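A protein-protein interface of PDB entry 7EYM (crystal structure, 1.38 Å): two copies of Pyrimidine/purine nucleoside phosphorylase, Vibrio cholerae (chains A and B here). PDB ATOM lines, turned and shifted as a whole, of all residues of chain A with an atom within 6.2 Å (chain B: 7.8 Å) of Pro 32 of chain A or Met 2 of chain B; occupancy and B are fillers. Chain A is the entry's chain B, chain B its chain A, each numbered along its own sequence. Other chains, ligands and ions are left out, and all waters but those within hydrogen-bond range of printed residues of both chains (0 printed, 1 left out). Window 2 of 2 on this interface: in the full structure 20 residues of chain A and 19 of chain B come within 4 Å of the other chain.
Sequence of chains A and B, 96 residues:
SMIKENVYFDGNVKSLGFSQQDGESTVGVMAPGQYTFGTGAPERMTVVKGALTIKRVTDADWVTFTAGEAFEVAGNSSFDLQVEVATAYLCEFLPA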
ATOM      1  N   GLY A  11     -32.302   7.608  14.376  1.00  0.00           N
ATOM      2  CA  GLY A  11     -32.831   6.374  14.916  1.00  0.00           C
ATOM      3  C   GLY A  11     -31.951   5.156  14.744  1.00  0.00           C
ATOM      4  O   GLY A  11     -32.345   4.066  15.180  1.00  0.00           O
ATOM      5  N   ASN A  12     -30.774   5.290  14.126  1.00  0.00           N
ATOM      6  CA  ASN A  12     -29.917   4.132  13.890  1.00  0.00           C
ATOM      7  C   ASN A  12     -29.048   3.762  15.085  1.00  0.00           C
ATOM      8  O   ASN A  12     -28.441   2.689  15.066  1.00  0.00           O
ATOM      9  CB  ASN A  12     -29.056   4.361  12.647  1.00  0.00           C
ATOM     10  CG  ASN A  12     -29.874   4.336  11.382  1.00  0.00           C
ATOM     11  OD1 ASN A  12     -30.544   3.351  11.091  1.00  0.00           O
ATOM     12  ND2 ASN A  12     -29.863   5.440  10.644  1.00  0.00           N
ATOM     13  N   MET A  30     -26.710  -0.441  17.879  1.00  0.00           N
ATOM     14  CA  MET A  30     -26.380   0.238  16.630  1.00  0.00           C
ATOM     15  C   MET A  30     -26.920  -0.592  15.482  1.00  0.00           C
ATOM     16  O   MET A  30     -26.601  -1.775  15.364  1.00  0.00           O
ATOM     17  CB  MET A  30     -24.870   0.412  16.493  1.00  0.00           C
ATOM     18  CG  MET A  30     -24.257   1.071  17.700  1.00  0.00           C
ATOM     19  SD  MET A  30     -22.534   1.510  17.385  1.00  0.00           S
ATOM     20  CE  MET A  30     -22.078   2.228  18.964  1.00  0.00           C
ATOM     21  N   ALA A  31     -27.738   0.034  14.641  1.00  0.00           N
ATOM     22  CA  ALA A  31     -28.215  -0.613  13.441  1.00  0.00           C
ATOM     23  C   ALA A  31     -27.082  -0.667  12.416  1.00  0.00           C
ATOM     24  O   ALA A  31     -26.097   0.073  12.526  1.00  0.00           O
ATOM     25  CB  ALA A  31     -29.391   0.180  12.874  1.00  0.00           C
ATOM     26  N   PRO A  32     -27.179  -1.553  11.429  1.00  0.00           N
ATOM     27  CA  PRO A  32     -26.135  -1.608  10.401  1.00  0.00           C
ATOM     28  C   PRO A  32     -25.908  -0.241   9.771  1.00  0.00           C
ATOM     29  O   PRO A  32     -26.846   0.518   9.501  1.00  0.00           O
ATOM     30  CB  PRO A  32     -26.687  -2.622   9.394  1.00  0.00           C
ATOM     31  CG  PRO A  32     -27.524  -3.549  10.249  1.00  0.00           C
ATOM     32  CD  PRO A  32     -28.200  -2.600  11.229  1.00  0.00           C
ATOM     33  N   GLY A  33     -24.639   0.087   9.576  1.00  0.00           N
ATOM     34  CA  GLY A  33     -24.263   1.389   9.071  1.00  0.00           C
ATOM     35  C   GLY A  33     -22.839   1.722   9.473  1.00  0.00           C
ATOM     36  O   GLY A  33     -22.092   0.872   9.955  1.00  0.00           O
ATOM     37  N   GLN A  34     -22.475   2.970   9.256  1.00  0.00           N
ATOM     38  CA  GLN A  34     -21.134   3.489   9.617  1.00  0.00           C
ATOM     39  C   GLN A  34     -21.301   4.802  10.373  1.00  0.00           C
ATOM     40  O   GLN A  34     -22.061   5.632   9.948  1.00  0.00           O
ATOM     41  CB  GLN A  34     -20.271   3.697   8.375  1.00  0.00           C
ATOM     42  CG  GLN A  34     -18.840   4.091   8.697  1.00  0.00           C
ATOM     43  CD  GLN A  34     -17.960   4.087   7.469  1.00  0.00           C
ATOM     44  OE1 GLN A  34     -18.233   4.761   6.495  1.00  0.00           O
ATOM     45  NE2 GLN A  34     -16.905   3.340   7.530  1.00  0.00           N
ATOM     46  N   TYR A  35     -20.648   4.918  11.528  1.00  0.00           N
ATOM     47  CA  TYR A  35     -20.884   6.000  12.473  1.00  0.00           C
ATOM     48  C   TYR A  35     -19.561   6.571  12.963  1.00  0.00           C
ATOM     49  O   TYR A  35     -18.541   5.882  12.977  1.00  0.00           O
ATOM     50  CB  TYR A  35     -21.682   5.472  13.678  1.00  0.00           C
ATOM     51  CG  TYR A  35     -22.907   4.712  13.259  1.00  0.00           C
ATOM     52  CD1 TYR A  35     -24.050   5.390  12.852  1.00  0.00           C
ATOM     53  CD2 TYR A  35     -22.920   3.319  13.229  1.00  0.00           C
ATOM     54  CE1 TYR A  35     -25.178   4.704  12.444  1.00  0.00           C
ATOM     55  CE2 TYR A  35     -24.047   2.623  12.826  1.00  0.00           C
ATOM     56  CZ  TYR A  35     -25.175   3.330  12.438  1.00  0.00           C
ATOM     57  OH  TYR A  35     -26.290   2.652  12.027  1.00  0.00           O
ATOM     58  N   VAL A  83     -20.913  -1.313  11.244  1.00  0.00           N
ATOM     59  CA  VAL A  83     -21.817  -2.277  11.848  1.00  0.00           C
ATOM     60  C   VAL A  83     -22.477  -2.997  10.684  1.00  0.00           C
ATOM     61  O   VAL A  83     -23.136  -2.351   9.862  1.00  0.00           O
ATOM     62  CB  VAL A  83     -22.863  -1.564  12.721  1.00  0.00           C
ATOM     63  CG1 VAL A  83     -23.739  -2.566  13.443  1.00  0.00           C
ATOM     64  CG2 VAL A  83     -22.176  -0.630  13.710  1.00  0.00           C
ATOM     65  N   GLU A  84     -22.283  -4.310  10.596  1.00  0.00           N
ATOM     66  CA  GLU A  84     -22.845  -5.089   9.499  1.00  0.00           C
ATOM     67  C   GLU A  84     -24.141  -5.790   9.868  1.00  0.00           C
ATOM     68  O   GLU A  84     -24.943  -6.091   8.979  1.00  0.00           O
ATOM     69  CB  GLU A  84     -21.828  -6.116   8.987  1.00  0.00           C
ATOM     70  CG  GLU A  84     -20.483  -5.506   8.597  1.00  0.00           C
ATOM     71  CD  GLU A  84     -20.588  -4.483   7.479  1.00  0.00           C
ATOM     72  OE1 GLU A  84     -21.528  -4.579   6.663  1.00  0.00           O
ATOM     73  OE2 GLU A  84     -19.721  -3.581   7.415  1.00  0.00           O
ATOM     74  N   VAL A  85     -24.346  -6.083  11.150  1.00  0.00           N
ATOM     75  CA  VAL A  85     -25.605  -6.594  11.678  1.00  0.00           C
ATOM     76  C   VAL A  85     -25.915  -5.769  12.917  1.00  0.00           C
ATOM     77  O   VAL A  85     -25.004  -5.283  13.592  1.00  0.00           O
ATOM     78  CB  VAL A  85     -25.525  -8.098  12.035  1.00  0.00           C
ATOM     79  CG1 VAL A  85     -25.131  -8.934  10.816  1.00  0.00           C
ATOM     80  CG2 VAL A  85     -24.562  -8.334  13.197  1.00  0.00           C
ATOM     81  N   ALA A  86     -27.203  -5.583  13.199  1.00  0.00           N
ATOM     82  CA  ALA A  86     -27.593  -4.803  14.378  1.00  0.00           C
ATOM     83  C   ALA A  86     -26.945  -5.398  15.620  1.00  0.00           C
ATOM     84  O   ALA A  86     -27.000  -6.610  15.841  1.00  0.00           O
ATOM     85  CB  ALA A  86     -29.109  -4.788  14.539  1.00  0.00           C
ATOM     86  N   THR A  87     -26.297  -4.536  16.407  1.00  0.00           N
ATOM     87  CA  THR A  87     -25.375  -4.974  17.442  1.00  0.00           C
ATOM     88  C   THR A  87     -25.690  -4.248  18.737  1.00  0.00           C
ATOM     89  O   THR A  87     -25.834  -3.020  18.751  1.00  0.00           O
ATOM     90  CB  THR A  87     -23.934  -4.709  16.992  1.00  0.00           C
ATOM     91  OG1 THR A  87     -23.593  -5.621  15.933  1.00  0.00           O
ATOM     92  CG2 THR A  87     -22.946  -4.886  18.153  1.00  0.00           C
ATOM     93  N   SER B   1     -38.193   1.932  14.222  1.00  0.00           N
ATOM     94  CA  SER B   1     -38.189   1.181  12.971  1.00  0.00           C
ATOM     95  C   SER B   1     -37.120   0.091  13.004  1.00  0.00           C
ATOM     96  O   SER B   1     -37.431  -1.089  13.190  1.00  0.00           O
ATOM     97  CB  SER B   1     -37.960   2.118  11.783  1.00  0.00           C
ATOM     98  OG  SER B   1     -38.468   1.558  10.579  1.00  0.00           O
ATOM     99  N   MET B   2     -35.858   0.480  12.828  1.00  0.00           N
ATOM    100  CA  MET B   2     -34.783  -0.492  12.951  1.00  0.00           C
ATOM    101  C   MET B   2     -34.651  -0.979  14.389  1.00  0.00           C
ATOM    102  O   MET B   2     -34.489  -2.180  14.630  1.00  0.00           O
ATOM    103  CB  MET B   2     -33.472   0.125  12.471  1.00  0.00           C
ATOM    104  CG  MET B   2     -33.460   0.455  10.987  1.00  0.00           C
ATOM    105  SD  MET B   2     -33.244  -1.031   9.994  1.00  0.00           S
ATOM    106  CE  MET B   2     -31.560  -1.413  10.372  1.00  0.00           C
ATOM    107  N   ILE B   3     -34.722  -0.061  15.350  1.00  0.00           N
ATOM    108  CA  ILE B   3     -34.513  -0.350  16.767  1.00  0.00           C
ATOM    109  C   ILE B   3     -35.789   0.049  17.489  1.00  0.00           C
ATOM    110  O   ILE B   3     -36.131   1.237  17.546  1.00  0.00           O
ATOM    111  CB  ILE B   3     -33.302   0.398  17.335  1.00  0.00           C
ATOM    112  CG1 ILE B   3     -32.061   0.143  16.478  1.00  0.00           C
ATOM    113  CG2 ILE B   3     -33.083   0.015  18.804  1.00  0.00           C
ATOM    114  CD1 ILE B   3     -30.891   1.065  16.782  1.00  0.00           C
ATOM    115  N   LYS B   4     -36.509  -0.923  18.027  1.00  0.00           N
ATOM    116  CA  LYS B   4     -37.811  -0.666  18.626  1.00  0.00           C
ATOM    117  C   LYS B   4     -37.656  -0.466  20.126  1.00  0.00           C
ATOM    118  O   LYS B   4     -37.190  -1.365  20.833  1.00  0.00           O
ATOM    119  CB  LYS B   4     -38.723  -1.862  18.377  1.00  0.00           C
ATOM    120  CG  LYS B   4     -40.098  -1.749  19.031  1.00  0.00           C
ATOM    121  CD  LYS B   4     -40.782  -0.442  18.642  1.00  0.00           C
ATOM    122  CE  LYS B   4     -42.109  -0.256  19.366  1.00  0.00           C
ATOM    123  NZ  LYS B   4     -42.957  -1.478  19.304  1.00  0.00           N
ATOM    124  N   GLU B   5     -38.057   0.695  20.624  1.00  0.00           N
ATOM    125  CA  GLU B   5     -38.065   0.925  22.061  1.00  0.00           C
ATOM    126  C   GLU B   5     -39.395   0.489  22.658  1.00  0.00           C
ATOM    127  O   GLU B   5     -40.464   0.820  22.131  1.00  0.00           O
ATOM    128  CB  GLU B   5     -37.809   2.388  22.406  1.00  0.00           C
ATOM    129  CG  GLU B   5     -37.610   2.569  23.909  1.00  0.00           C
ATOM    130  CD  GLU B   5     -37.862   3.980  24.408  1.00  0.00           C
ATOM    131  OE1 GLU B   5     -37.279   4.343  25.457  1.00  0.00           O
ATOM    132  OE2 GLU B   5     -38.647   4.715  23.776  1.00  0.00           O
ATOM    133  N   LEU B  16     -34.760  -2.281  24.045  1.00  0.00           N
ATOM    134  CA  LEU B  16     -34.505  -1.989  22.640  1.00  0.00           C
ATOM    135  C   LEU B  16     -34.481  -3.295  21.861  1.00  0.00           C
ATOM    136  O   LEU B  16     -33.635  -4.164  22.120  1.00  0.00           O
ATOM    137  CB  LEU B  16     -33.170  -1.265  22.507  1.00  0.00           C
ATOM    138  CG  LEU B  16     -33.037   0.068  23.254  1.00  0.00           C
ATOM    139  CD1 LEU B  16     -31.593   0.530  23.230  1.00  0.00           C
ATOM    140  CD2 LEU B  16     -33.959   1.130  22.659  1.00  0.00           C
ATOM    141  N   GLY B  17     -35.415  -3.447  20.927  1.00  0.00           N
ATOM    142  CA  GLY B  17     -35.485  -4.641  20.106  1.00  0.00           C
ATOM    143  C   GLY B  17     -34.747  -4.420  18.796  1.00  0.00           C
ATOM    144  O   GLY B  17     -34.878  -3.372  18.161  1.00  0.00           O
ATOM    145  N   PHE B  18     -33.972  -5.420  18.397  1.00  0.00           N
ATOM    146  CA  PHE B  18     -33.145  -5.308  17.210  1.00  0.00           C
ATOM    147  C   PHE B  18     -33.122  -6.651  16.501  1.00  0.00           C
ATOM    148  O   PHE B  18     -33.204  -7.707  17.129  1.00  0.00           O
ATOM    149  CB  PHE B  18     -31.719  -4.819  17.541  1.00  0.00           C
ATOM    150  CG  PHE B  18     -30.944  -5.725  18.476  1.00  0.00           C
ATOM    151  CD1 PHE B  18     -31.194  -5.718  19.848  1.00  0.00           C
ATOM    152  CD2 PHE B  18     -29.960  -6.580  17.984  1.00  0.00           C
ATOM    153  CE1 PHE B  18     -30.478  -6.551  20.707  1.00  0.00           C
ATOM    154  CE2 PHE B  18     -29.234  -7.417  18.835  1.00  0.00           C
ATOM    155  CZ  PHE B  18     -29.494  -7.400  20.207  1.00  0.00           C
ATOM    156  N   SER B  19     -32.952  -6.605  15.189  1.00  0.00           N
ATOM    157  CA  SER B  19     -33.050  -7.809  14.385  1.00  0.00           C
ATOM    158  C   SER B  19     -31.709  -8.136  13.747  1.00  0.00           C
ATOM    159  O   SER B  19     -31.023  -7.253  13.219  1.00  0.00           O
ATOM    160  CB  SER B  19     -34.135  -7.671  13.302  1.00  0.00           C
ATOM    161  OG  SER B  19     -35.358  -7.184  13.845  1.00  0.00           O
ATOM    162  N   GLN B  20     -31.358  -9.410  13.803  1.00  0.00           N
ATOM    163  CA  GLN B  20     -30.282  -9.991  13.030  1.00  0.00           C
ATOM    164  C   GLN B  20     -30.942 -10.875  11.971  1.00  0.00           C
ATOM    165  O   GLN B  20     -32.165 -10.893  11.838  1.00  0.00           O
ATOM    166  CB  GLN B  20     -29.294 -10.701  13.962  1.00  0.00           C
ATOM    167  CG  GLN B  20     -28.810  -9.767  15.101  1.00  0.00           C
ATOM    168  CD  GLN B  20     -27.636 -10.306  15.910  1.00  0.00           C
ATOM    169  OE1 GLN B  20     -27.486 -11.514  16.083  1.00  0.00           O
ATOM    170  NE2 GLN B  20     -26.800  -9.396  16.429  1.00  0.00           N
ATOM    171  N   GLU B  24     -35.142 -11.404  15.919  1.00  0.00           N
ATOM    172  CA  GLU B  24     -35.075 -10.317  16.889  1.00  0.00           C
ATOM    173  C   GLU B  24     -34.521 -10.758  18.240  1.00  0.00           C
ATOM    174  O   GLU B  24     -34.757 -11.877  18.702  1.00  0.00           O
ATOM    175  CB  GLU B  24     -36.462  -9.693  17.080  1.00  0.00           C
ATOM    176  CG  GLU B  24     -36.426  -8.279  17.642  1.00  0.00           C
ATOM    177  CD  GLU B  24     -37.794  -7.644  17.751  1.00  0.00           C
ATOM    178  OE1 GLU B  24     -38.805  -8.337  17.517  1.00  0.00           O
ATOM    179  OE2 GLU B  24     -37.865  -6.431  18.041  1.00  0.00           O
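No position is printed for both chains.
Printed residues of chain B within 4 Å of Gly 11 of chain A: Ile 3.
Of chain B, only Met 2 comes within 4 Å of Pro 32 of chain A.
Val 83 of chain A touches none of the printed residues of chain B.
Of the printed residues of chain B, Ala 86 of chain A touches Phe 18 (3.7 Å), Ser 19 (3.4 Å) and Gln 20 (2.9 Å).
Printed residues of chain A within 4 Å of Met 2 of chain B: Ala 31 and Pro 32.
Of the 11 printed residues of chain B, 5 touch a printed residue of chain A.
Printed residues of chain B that touch a printed residue of chain A: Met 2, Ile 3, Phe 18, Ser 19 and Gln 20.
Hydrophobic or aromatic side chains of chain A within 4 Å of the printed part of chain B: Ala 31, Pro 32 and Ala 86.
Among the printed residues, 8 pairs touch across the chains.
Among the printed residues, no Asp or Glu carboxylate lies within 4 Å of a Lys or Arg side-chain nitrogen of the other chain.
Gly 11 of chain A touches Ile 3 of chain B.
CD1 of Ile 3 of chain B touches O of Asn 12 of chain A (3.4 Å).
CE of Met 2 of chain B touches CB of Ala 31 of chain A, 3.7 Å away.
CD1 of Ile 3 of chain B touches N of Ala 31 of chain A, 3.9 Å away.
Pro 32 of chain A touches Met 2 of chain B.
O of Ala 86 of chain A touches CD2 of Phe 18 of chain B (3.7 Å).
Ser 19 of chain B touches Ala 86 of chain A (O to CB, 3.4 Å).
The side-chain amide nitrogen (NE2) of Gln 20 of chain B is in hydrogen-bond range of the backbone carbonyl oxygen (O) of Ala 86 of chain A.
O of Pro 32 of chain A sits at hydrogen-bond distance from OH of Tyr 35 of chain A (3.4 Å).
The backbone carbonyl oxygen (O) of Ala 31 of chain A sits at hydrogen-bond distance from the side-chain hydroxyl (OH) of Tyr 35 of chain A, 2.6 Å away.
O of Asn 12 of chain A lies within hydrogen-bond range of N of Ala 31 of chain A (2.8 Å).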
